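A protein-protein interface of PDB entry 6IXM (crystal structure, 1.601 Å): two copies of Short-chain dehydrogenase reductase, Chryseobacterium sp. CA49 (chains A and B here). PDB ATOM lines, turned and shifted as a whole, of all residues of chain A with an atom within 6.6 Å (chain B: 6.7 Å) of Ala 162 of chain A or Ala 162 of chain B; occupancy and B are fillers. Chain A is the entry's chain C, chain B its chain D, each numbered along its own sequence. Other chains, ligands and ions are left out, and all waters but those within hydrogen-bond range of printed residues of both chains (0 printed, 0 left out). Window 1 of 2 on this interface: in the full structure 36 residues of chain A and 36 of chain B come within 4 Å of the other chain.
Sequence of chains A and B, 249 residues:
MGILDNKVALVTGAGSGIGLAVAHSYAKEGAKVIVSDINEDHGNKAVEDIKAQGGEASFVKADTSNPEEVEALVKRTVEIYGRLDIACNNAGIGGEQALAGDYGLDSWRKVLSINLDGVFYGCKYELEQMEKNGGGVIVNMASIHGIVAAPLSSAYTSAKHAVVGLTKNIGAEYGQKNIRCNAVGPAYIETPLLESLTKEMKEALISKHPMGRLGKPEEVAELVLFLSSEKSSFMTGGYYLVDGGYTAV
O of Gly 146 of chain B sits close to ND1 of His 161 of chain B (3.3 Å).
The side-chain hydroxyl (OG) of Ser 158 of chain B sits at hydrogen-bond distance from the backbone carbonyl oxygen (O) of Ser 154 of chain B (2.9 Å).
OG of Ser 158 of chain A lies within hydrogen-bond range of O of Ser 154 of chain A (2.8 Å).
A ring nitrogen (ND1) of His 161 of chain A lies within hydrogen-bond range of the backbone carbonyl oxygen (O) of Thr 157 of chain A (3.0 Å).
A ring nitrogen (ND1) of His 161 of chain B is in hydrogen-bond range of the backbone carbonyl oxygen (O) of Thr 157 of chain B, 3.0 Å away.
The backbone carbonyl oxygen (O) of Gly 146 of chain A sits close to a ring nitrogen (ND1) of His 161 of chain A, 3.3 Å away.
Among the printed residues, merely in contact across the chains: Ser 158 of chain A with Ala 162 of chain B, Ala 162 of chain A with Ser 158 of chain B, His 161 of chain A with His 161 of chain B, Leu 166 of chain A with Ser 158 of chain B, Ser 158 of chain A with Leu 166 of chain B, His 161 of chain A with Gly 165 of chain B, Gly 165 of chain A with His 161 of chain B, Thr 157 of chain A with Gly 165 of chain B, Leu 112 of chain A with Leu 116 of chain B, Leu 116 of chain A with Leu 112 of chain B, Gly 165 of chain A with Thr 157 of chain B, Trp 108 of chain A with Leu 116 of chain B, Leu 116 of chain A with Trp 108 of chain B, Leu 166 of chain A with Ser 154 of chain B, Ala 162 of chain A with Ala 162 of chain B and Ala 162 of chain A with His 161 of chain B.
Of the printed residues of chain B, Leu 116 of chain A touches Trp 108 (3.9 Å) and Leu 112 (3.6 Å).
Of the printed residues of chain B, Thr 157 of chain A touches Gly 165.
Lys 160 of chain A touches none of the printed residues of chain B.
Printed residues of chain B within 4 Å of Ala 162 of chain A: Ser 158, His 161 and Ala 162.
Printed residues of chain B within 4 Å of Leu 166 of chain A: Ser 154 (3.9 Å) and Ser 158 (3.3 Å).
Thr 167 of chain A touches none of the printed residues of chain B.
Printed residues of chain A within 4 Å of Leu 112 of chain B: Leu 116 (3.6 Å).
Of chain A, only Ser 158 and Ala 162 come within 4 Å of Ala 162 of chain B.
Printed residues of chain A within 4 Å of Gly 165 of chain B: Thr 157 and His 161.
The nearest printed residue of chain B that does not touch Ala 162 of chain A is Ala 159 of chain B (5.0 Å).
The nearest printed residue of chain B that does not touch His 161 of chain A is Ala 162 of chain B (4.1 Å).
Of the 16 printed residues of chain A, 9 touch a printed residue of chain B.
Hydrophobic or aromatic side chains of chain A that line the printed part of chain B: Trp 108, Leu 112, Leu 116, His 161, Ala 162 and Leu 166.
Among the printed residues, 16 pairs touch across the chains.
Trp 108 of chain A touches Leu 116 of chain B, and with the chains exchanged Leu 116 of chain A touches Trp 108 of chain B.
Thr 157 of chain A touches Gly 165 of chain B, and with the chains exchanged Gly 165 of chain A touches Thr 157 of chain B.
His 161 of chain A touches its own counterpart, His 161 of chain B.
Ala 162 of chain B touches its own counterpart, Ala 162 of chain A.
Positions printed for both chains: 108, 112, 116, 146, 154, 157, 158, 159, 160, 161, 162, 163, 164, 165, 166 and 167.
Of the 16 pairs that touch across the chains among the printed residues, 14 have their exchanged pair printed and touching as well.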
ATOM      1  N   TRP A 108      16.840 -32.920  -2.681  1.00  0.00           N
ATOM      2  CA  TRP A 108      15.981 -31.986  -3.406  1.00  0.00           C
ATOM      3  C   TRP A 108      15.801 -32.428  -4.854  1.00  0.00           C
ATOM      4  O   TRP A 108      14.671 -32.537  -5.353  1.00  0.00           O
ATOM      5  CB  TRP A 108      16.563 -30.560  -3.358  1.00  0.00           C
ATOM      6  CG  TRP A 108      15.720 -29.565  -4.123  1.00  0.00           C
ATOM      7  CD1 TRP A 108      15.854 -29.204  -5.431  1.00  0.00           C
ATOM      8  CD2 TRP A 108      14.606 -28.825  -3.615  1.00  0.00           C
ATOM      9  NE1 TRP A 108      14.881 -28.288  -5.776  1.00  0.00           N
ATOM     10  CE2 TRP A 108      14.107 -28.036  -4.675  1.00  0.00           C
ATOM     11  CE3 TRP A 108      13.987 -28.746  -2.362  1.00  0.00           C
ATOM     12  CZ2 TRP A 108      13.016 -27.182  -4.521  1.00  0.00           C
ATOM     13  CZ3 TRP A 108      12.898 -27.893  -2.210  1.00  0.00           C
ATOM     14  CH2 TRP A 108      12.423 -27.132  -3.284  1.00  0.00           C
ATOM     15  N   LEU A 112      12.185 -33.783  -6.516  1.00  0.00           N
ATOM     16  CA  LEU A 112      11.544 -33.027  -7.582  1.00  0.00           C
ATOM     17  C   LEU A 112      11.560 -33.790  -8.899  1.00  0.00           C
ATOM     18  O   LEU A 112      10.625 -33.649  -9.696  1.00  0.00           O
ATOM     19  CB  LEU A 112      12.211 -31.658  -7.745  1.00  0.00           C
ATOM     20  CG  LEU A 112      11.593 -30.502  -6.940  1.00  0.00           C
ATOM     21  CD1 LEU A 112      10.174 -30.153  -7.410  1.00  0.00           C
ATOM     22  CD2 LEU A 112      11.596 -30.794  -5.431  1.00  0.00           C
ATOM     23  N   LEU A 116       7.693 -34.340  -9.417  1.00  0.00           N
ATOM     24  CA  LEU A 116       7.218 -33.341 -10.368  1.00  0.00           C
ATOM     25  C   LEU A 116       7.590 -33.687 -11.803  1.00  0.00           C
ATOM     26  O   LEU A 116       6.691 -33.848 -12.632  1.00  0.00           O
ATOM     27  CB  LEU A 116       7.727 -31.933 -10.015  1.00  0.00           C
ATOM     28  CG  LEU A 116       7.354 -30.888 -11.077  1.00  0.00           C
ATOM     29  CD1 LEU A 116       5.819 -30.771 -11.315  1.00  0.00           C
ATOM     30  CD2 LEU A 116       7.976 -29.538 -10.719  1.00  0.00           C
ATOM     31  N   GLY A 146       0.220 -30.553  -1.309  1.00  0.00           N
ATOM     32  CA  GLY A 146       0.057 -29.618  -2.403  1.00  0.00           C
ATOM     33  C   GLY A 146      -0.601 -28.308  -2.003  1.00  0.00           C
ATOM     34  O   GLY A 146      -0.605 -27.372  -2.810  1.00  0.00           O
ATOM     35  N   SER A 154      10.478 -30.197   2.724  1.00  0.00           N
ATOM     36  CA  SER A 154      10.229 -29.048   1.854  1.00  0.00           C
ATOM     37  C   SER A 154      10.252 -29.429   0.379  1.00  0.00           C
ATOM     38  O   SER A 154       9.497 -28.850  -0.410  1.00  0.00           O
ATOM     39  CB  SER A 154      11.237 -27.934   2.146  1.00  0.00           C
ATOM     40  OG  SER A 154      12.556 -28.377   1.906  1.00  0.00           O
ATOM     41  N   THR A 157       6.774 -31.009  -0.396  1.00  0.00           N
ATOM     42  CA  THR A 157       5.739 -29.978  -0.437  1.00  0.00           C
ATOM     43  C   THR A 157       5.837 -29.152  -1.707  1.00  0.00           C
ATOM     44  O   THR A 157       4.821 -28.840  -2.344  1.00  0.00           O
ATOM     45  CB  THR A 157       5.877 -29.076   0.785  1.00  0.00           C
ATOM     46  OG1 THR A 157       5.755 -29.884   1.964  1.00  0.00           O
ATOM     47  CG2 THR A 157       4.814 -27.974   0.777  1.00  0.00           C
ATOM     48  N   SER A 158       7.059 -28.769  -2.075  1.00  0.00           N
ATOM     49  CA  SER A 158       7.250 -27.972  -3.283  1.00  0.00           C
ATOM     50  C   SER A 158       6.816 -28.755  -4.523  1.00  0.00           C
ATOM     51  O   SER A 158       6.127 -28.225  -5.405  1.00  0.00           O
ATOM     52  CB  SER A 158       8.712 -27.548  -3.396  1.00  0.00           C
ATOM     53  OG  SER A 158       9.140 -26.790  -2.253  1.00  0.00           O
ATOM     54  N   ALA A 159       7.220 -30.025  -4.614  1.00  0.00           N
ATOM     55  CA  ALA A 159       6.838 -30.841  -5.764  1.00  0.00           C
ATOM     56  C   ALA A 159       5.332 -31.025  -5.841  1.00  0.00           C
ATOM     57  O   ALA A 159       4.748 -30.944  -6.927  1.00  0.00           O
ATOM     58  CB  ALA A 159       7.532 -32.199  -5.691  1.00  0.00           C
ATOM     59  N   LYS A 160       4.678 -31.264  -4.700  1.00  0.00           N
ATOM     60  CA  LYS A 160       3.243 -31.537  -4.728  1.00  0.00           C
ATOM     61  C   LYS A 160       2.444 -30.273  -5.021  1.00  0.00           C
ATOM     62  O   LYS A 160       1.428 -30.326  -5.720  1.00  0.00           O
ATOM     63  CB  LYS A 160       2.807 -32.171  -3.407  1.00  0.00           C
ATOM     64  CG  LYS A 160       3.375 -33.584  -3.205  1.00  0.00           C
ATOM     65  CD  LYS A 160       2.953 -34.528  -4.325  1.00  0.00           C
ATOM     66  CE  LYS A 160       3.181 -35.994  -3.956  1.00  0.00           C
ATOM     67  NZ  LYS A 160       2.690 -36.940  -5.017  1.00  0.00           N
ATOM     68  N   HIS A 161       2.888 -29.123  -4.498  1.00  0.00           N
ATOM     69  CA  HIS A 161       2.336 -27.847  -4.942  1.00  0.00           C
ATOM     70  C   HIS A 161       2.452 -27.705  -6.455  1.00  0.00           C
ATOM     71  O   HIS A 161       1.492 -27.309  -7.129  1.00  0.00           O
ATOM     72  CB  HIS A 161       3.062 -26.688  -4.250  1.00  0.00           C
ATOM     73  CG  HIS A 161       2.451 -26.274  -2.943  1.00  0.00           C
ATOM     74  ND1 HIS A 161       2.489 -27.070  -1.816  1.00  0.00           N
ATOM     75  CD2 HIS A 161       1.822 -25.132  -2.581  1.00  0.00           C
ATOM     76  CE1 HIS A 161       1.881 -26.444  -0.821  1.00  0.00           C
ATOM     77  NE2 HIS A 161       1.476 -25.261  -1.256  1.00  0.00           N
ATOM     78  N   ALA A 162       3.634 -28.017  -7.003  1.00  0.00           N
ATOM     79  CA  ALA A 162       3.830 -27.900  -8.449  1.00  0.00           C
ATOM     80  C   ALA A 162       2.863 -28.800  -9.223  1.00  0.00           C
ATOM     81  O   ALA A 162       2.363 -28.416 -10.290  1.00  0.00           O
ATOM     82  CB  ALA A 162       5.284 -28.218  -8.810  1.00  0.00           C
ATOM     83  N   VAL A 163       2.567 -29.988  -8.694  1.00  0.00           N
ATOM     84  CA  VAL A 163       1.629 -30.884  -9.376  1.00  0.00           C
ATOM     85  C   VAL A 163       0.239 -30.260  -9.439  1.00  0.00           C
ATOM     86  O   VAL A 163      -0.466 -30.372 -10.454  1.00  0.00           O
ATOM     87  CB  VAL A 163       1.615 -32.259  -8.685  1.00  0.00           C
ATOM     88  CG1 VAL A 163       0.449 -33.123  -9.176  1.00  0.00           C
ATOM     89  CG2 VAL A 163       2.953 -32.975  -8.914  1.00  0.00           C
ATOM     90  N   VAL A 164      -0.169 -29.571  -8.372  1.00  0.00           N
ATOM     91  CA  VAL A 164      -1.456 -28.881  -8.390  1.00  0.00           C
ATOM     92  C   VAL A 164      -1.483 -27.843  -9.502  1.00  0.00           C
ATOM     93  O   VAL A 164      -2.458 -27.744 -10.259  1.00  0.00           O
ATOM     94  CB  VAL A 164      -1.733 -28.249  -7.015  1.00  0.00           C
ATOM     95  CG1 VAL A 164      -2.991 -27.425  -7.081  1.00  0.00           C
ATOM     96  CG2 VAL A 164      -1.866 -29.330  -5.969  1.00  0.00           C
ATOM     97  N   GLY A 165      -0.397 -27.073  -9.635  1.00  0.00           N
ATOM     98  CA  GLY A 165      -0.351 -26.041 -10.660  1.00  0.00           C
ATOM     99  C   GLY A 165      -0.367 -26.619 -12.060  1.00  0.00           C
ATOM    100  O   GLY A 165      -1.093 -26.136 -12.938  1.00  0.00           O
ATOM    101  N   LEU A 166       0.460 -27.640 -12.289  1.00  0.00           N
ATOM    102  CA  LEU A 166       0.472 -28.339 -13.572  1.00  0.00           C
ATOM    103  C   LEU A 166      -0.916 -28.846 -13.938  1.00  0.00           C
ATOM    104  O   LEU A 166      -1.345 -28.731 -15.094  1.00  0.00           O
ATOM    105  CB  LEU A 166       1.460 -29.502 -13.503  1.00  0.00           C
ATOM    106  CG  LEU A 166       1.487 -30.399 -14.736  1.00  0.00           C
ATOM    107  CD1 LEU A 166       1.951 -29.600 -15.959  1.00  0.00           C
ATOM    108  CD2 LEU A 166       2.382 -31.621 -14.493  1.00  0.00           C
ATOM    109  N   THR A 167      -1.633 -29.410 -12.955  1.00  0.00           N
ATOM    110  CA  THR A 167      -2.989 -29.908 -13.192  1.00  0.00           C
ATOM    111  C   THR A 167      -3.942 -28.787 -13.614  1.00  0.00           C
ATOM    112  O   THR A 167      -4.758 -28.963 -14.536  1.00  0.00           O
ATOM    113  CB  THR A 167      -3.494 -30.606 -11.925  1.00  0.00           C
ATOM    114  OG1 THR A 167      -2.647 -31.718 -11.633  1.00  0.00           O
ATOM    115  CG2 THR A 167      -4.923 -31.099 -12.100  1.00  0.00           C
ATOM    116  N   TRP B 108      11.280 -27.249 -20.188  1.00  0.00           N
ATOM    117  CA  TRP B 108      10.684 -27.502 -18.877  1.00  0.00           C
ATOM    118  C   TRP B 108      11.735 -27.441 -17.774  1.00  0.00           C
ATOM    119  O   TRP B 108      11.558 -26.748 -16.767  1.00  0.00           O
ATOM    120  CB  TRP B 108       9.989 -28.872 -18.879  1.00  0.00           C
ATOM    121  CG  TRP B 108       9.525 -29.310 -17.502  1.00  0.00           C
ATOM    122  CD1 TRP B 108      10.251 -29.984 -16.569  1.00  0.00           C
ATOM    123  CD2 TRP B 108       8.232 -29.089 -16.924  1.00  0.00           C
ATOM    124  NE1 TRP B 108       9.490 -30.194 -15.433  1.00  0.00           N
ATOM    125  CE2 TRP B 108       8.247 -29.655 -15.633  1.00  0.00           C
ATOM    126  CE3 TRP B 108       7.065 -28.466 -17.376  1.00  0.00           C
ATOM    127  CZ2 TRP B 108       7.132 -29.616 -14.783  1.00  0.00           C
ATOM    128  CZ3 TRP B 108       5.961 -28.436 -16.534  1.00  0.00           C
ATOM    129  CH2 TRP B 108       6.013 -28.998 -15.251  1.00  0.00           C
ATOM    130  N   LEU B 112      12.149 -24.677 -14.520  1.00  0.00           N
ATOM    131  CA  LEU B 112      12.165 -25.130 -13.134  1.00  0.00           C
ATOM    132  C   LEU B 112      13.503 -24.846 -12.471  1.00  0.00           C
ATOM    133  O   LEU B 112      13.534 -24.504 -11.283  1.00  0.00           O
ATOM    134  CB  LEU B 112      11.851 -26.626 -13.051  1.00  0.00           C
ATOM    135  CG  LEU B 112      10.380 -27.018 -12.848  1.00  0.00           C
ATOM    136  CD1 LEU B 112       9.880 -26.539 -11.496  1.00  0.00           C
ATOM    137  CD2 LEU B 112       9.484 -26.491 -13.963  1.00  0.00           C
ATOM    138  N   LEU B 116      12.396 -22.330  -9.702  1.00  0.00           N
ATOM    139  CA  LEU B 116      12.227 -23.068  -8.458  1.00  0.00           C
ATOM    140  C   LEU B 116      13.563 -23.425  -7.822  1.00  0.00           C
ATOM    141  O   LEU B 116      13.812 -23.030  -6.680  1.00  0.00           O
ATOM    142  CB  LEU B 116      11.383 -24.338  -8.673  1.00  0.00           C
ATOM    143  CG  LEU B 116      11.374 -25.245  -7.437  1.00  0.00           C
ATOM    144  CD1 LEU B 116      10.765 -24.556  -6.193  1.00  0.00           C
ATOM    145  CD2 LEU B 116      10.659 -26.571  -7.730  1.00  0.00           C
ATOM    146  N   GLY B 146       1.433 -18.790  -9.104  1.00  0.00           N
ATOM    147  CA  GLY B 146       1.535 -19.690  -7.973  1.00  0.00           C
ATOM    148  C   GLY B 146       0.201 -20.194  -7.440  1.00  0.00           C
ATOM    149  O   GLY B 146       0.200 -21.091  -6.588  1.00  0.00           O
ATOM    150  N   SER B 154       2.970 -23.976 -18.605  1.00  0.00           N
ATOM    151  CA  SER B 154       2.812 -24.938 -17.512  1.00  0.00           C
ATOM    152  C   SER B 154       4.064 -25.042 -16.645  1.00  0.00           C
ATOM    153  O   SER B 154       3.952 -25.265 -15.438  1.00  0.00           O
ATOM    154  CB  SER B 154       2.439 -26.315 -18.051  1.00  0.00           C
ATOM    155  OG  SER B 154       3.397 -26.761 -18.992  1.00  0.00           O
ATOM    156  N   TYR B 156       6.260 -22.643 -15.897  1.00  0.00           N
ATOM    157  CA  TYR B 156       6.275 -21.471 -15.031  1.00  0.00           C
ATOM    158  C   TYR B 156       5.256 -21.608 -13.907  1.00  0.00           C
ATOM    159  O   TYR B 156       5.567 -21.351 -12.734  1.00  0.00           O
ATOM    160  CB  TYR B 156       6.003 -20.224 -15.879  1.00  0.00           C
ATOM    161  CG  TYR B 156       6.083 -18.907 -15.140  1.00  0.00           C
ATOM    162  CD1 TYR B 156       4.959 -18.337 -14.569  1.00  0.00           C
ATOM    163  CD2 TYR B 156       7.284 -18.225 -15.033  1.00  0.00           C
ATOM    164  CE1 TYR B 156       5.025 -17.128 -13.905  1.00  0.00           C
ATOM    165  CE2 TYR B 156       7.355 -17.007 -14.376  1.00  0.00           C
ATOM    166  CZ  TYR B 156       6.219 -16.468 -13.813  1.00  0.00           C
ATOM    167  OH  TYR B 156       6.274 -15.263 -13.144  1.00  0.00           O
ATOM    168  N   THR B 157       4.031 -22.021 -14.247  1.00  0.00           N
ATOM    169  CA  THR B 157       2.996 -22.201 -13.231  1.00  0.00           C
ATOM    170  C   THR B 157       3.420 -23.243 -12.204  1.00  0.00           C
ATOM    171  O   THR B 157       3.229 -23.064 -10.994  1.00  0.00           O
ATOM    172  CB  THR B 157       1.682 -22.613 -13.906  1.00  0.00           C
ATOM    173  OG1 THR B 157       1.300 -21.600 -14.851  1.00  0.00           O
ATOM    174  CG2 THR B 157       0.560 -22.802 -12.894  1.00  0.00           C
ATOM    175  N   SER B 158       3.983 -24.352 -12.675  1.00  0.00           N
ATOM    176  CA  SER B 158       4.415 -25.404 -11.771  1.00  0.00           C
ATOM    177  C   SER B 158       5.517 -24.893 -10.848  1.00  0.00           C
ATOM    178  O   SER B 158       5.486 -25.111  -9.634  1.00  0.00           O
ATOM    179  CB  SER B 158       4.912 -26.588 -12.598  1.00  0.00           C
ATOM    180  OG  SER B 158       3.818 -27.180 -13.297  1.00  0.00           O
ATOM    181  N   ALA B 159       6.493 -24.176 -11.414  1.00  0.00           N
ATOM    182  CA  ALA B 159       7.585 -23.644 -10.605  1.00  0.00           C
ATOM    183  C   ALA B 159       7.074 -22.658  -9.566  1.00  0.00           C
ATOM    184  O   ALA B 159       7.507 -22.691  -8.406  1.00  0.00           O
ATOM    185  CB  ALA B 159       8.629 -22.975 -11.498  1.00  0.00           C
ATOM    186  N   LYS B 160       6.155 -21.772  -9.960  1.00  0.00           N
ATOM    187  CA  LYS B 160       5.686 -20.745  -9.031  1.00  0.00           C
ATOM    188  C   LYS B 160       4.785 -21.341  -7.948  1.00  0.00           C
ATOM    189  O   LYS B 160       4.835 -20.909  -6.793  1.00  0.00           O
ATOM    190  CB  LYS B 160       4.976 -19.626  -9.800  1.00  0.00           C
ATOM    191  CG  LYS B 160       5.917 -18.816 -10.692  1.00  0.00           C
ATOM    192  CD  LYS B 160       7.075 -18.244  -9.892  1.00  0.00           C
ATOM    193  CE  LYS B 160       7.841 -17.221 -10.741  1.00  0.00           C
ATOM    194  NZ  LYS B 160       8.618 -16.283  -9.892  1.00  0.00           N
ATOM    195  N   HIS B 161       3.958 -22.337  -8.294  1.00  0.00           N
ATOM    196  CA  HIS B 161       3.257 -23.094  -7.262  1.00  0.00           C
ATOM    197  C   HIS B 161       4.246 -23.697  -6.270  1.00  0.00           C
ATOM    198  O   HIS B 161       4.045 -23.637  -5.049  1.00  0.00           O
ATOM    199  CB  HIS B 161       2.411 -24.205  -7.907  1.00  0.00           C
ATOM    200  CG  HIS B 161       1.024 -23.783  -8.275  1.00  0.00           C
ATOM    201  ND1 HIS B 161       0.755 -22.891  -9.294  1.00  0.00           N
ATOM    202  CD2 HIS B 161      -0.180 -24.165  -7.782  1.00  0.00           C
ATOM    203  CE1 HIS B 161      -0.551 -22.715  -9.388  1.00  0.00           C
ATOM    204  NE2 HIS B 161      -1.141 -23.480  -8.487  1.00  0.00           N
ATOM    205  N   ALA B 162       5.325 -24.293  -6.779  1.00  0.00           N
ATOM    206  CA  ALA B 162       6.318 -24.894  -5.893  1.00  0.00           C
ATOM    207  C   ALA B 162       6.946 -23.856  -4.969  1.00  0.00           C
ATOM    208  O   ALA B 162       7.237 -24.148  -3.800  1.00  0.00           O
ATOM    209  CB  ALA B 162       7.392 -25.602  -6.719  1.00  0.00           C
ATOM    210  N   VAL B 163       7.158 -22.630  -5.462  1.00  0.00           N
ATOM    211  CA  VAL B 163       7.724 -21.583  -4.606  1.00  0.00           C
ATOM    212  C   VAL B 163       6.775 -21.267  -3.455  1.00  0.00           C
ATOM    213  O   VAL B 163       7.204 -21.024  -2.318  1.00  0.00           O
ATOM    214  CB  VAL B 163       8.042 -20.327  -5.441  1.00  0.00           C
ATOM    215  CG1 VAL B 163       8.369 -19.137  -4.525  1.00  0.00           C
ATOM    216  CG2 VAL B 163       9.217 -20.597  -6.374  1.00  0.00           C
ATOM    217  N   VAL B 164       5.471 -21.275  -3.725  1.00  0.00           N
ATOM    218  CA  VAL B 164       4.498 -21.054  -2.658  1.00  0.00           C
ATOM    219  C   VAL B 164       4.625 -22.139  -1.595  1.00  0.00           C
ATOM    220  O   VAL B 164       4.650 -21.852  -0.390  1.00  0.00           O
ATOM    221  CB  VAL B 164       3.077 -20.977  -3.247  1.00  0.00           C
ATOM    222  CG1 VAL B 164       2.034 -20.934  -2.150  1.00  0.00           C
ATOM    223  CG2 VAL B 164       2.958 -19.749  -4.183  1.00  0.00           C
ATOM    224  N   GLY B 165       4.724 -23.401  -2.025  1.00  0.00           N
ATOM    225  CA  GLY B 165       4.843 -24.485  -1.066  1.00  0.00           C
ATOM    226  C   GLY B 165       6.127 -24.413  -0.263  1.00  0.00           C
ATOM    227  O   GLY B 165       6.123 -24.624   0.955  1.00  0.00           O
ATOM    228  N   LEU B 166       7.242 -24.116  -0.938  1.00  0.00           N
ATOM    229  CA  LEU B 166       8.515 -23.982  -0.242  1.00  0.00           C
ATOM    230  C   LEU B 166       8.437 -22.897   0.819  1.00  0.00           C
ATOM    231  O   LEU B 166       8.963 -23.057   1.929  1.00  0.00           O
ATOM    232  CB  LEU B 166       9.618 -23.656  -1.250  1.00  0.00           C
ATOM    233  CG  LEU B 166      10.994 -23.326  -0.700  1.00  0.00           C
ATOM    234  CD1 LEU B 166      11.609 -24.513   0.030  1.00  0.00           C
ATOM    235  CD2 LEU B 166      11.873 -22.837  -1.838  1.00  0.00           C
ATOM    236  N   THR B 167       7.772 -21.785   0.482  1.00  0.00           N
ATOM    237  CA  THR B 167       7.629 -20.671   1.409  1.00  0.00           C
ATOM    238  C   THR B 167       6.829 -21.076   2.643  1.00  0.00           C
ATOM    239  O   THR B 167       7.179 -20.708   3.771  1.00  0.00           O
ATOM    240  CB  THR B 167       6.954 -19.507   0.686  1.00  0.00           C
ATOM    241  OG1 THR B 167       7.774 -19.076  -0.415  1.00  0.00           O
ATOM    242  CG2 THR B 167       6.713 -18.346   1.621  1.00  0.00           C
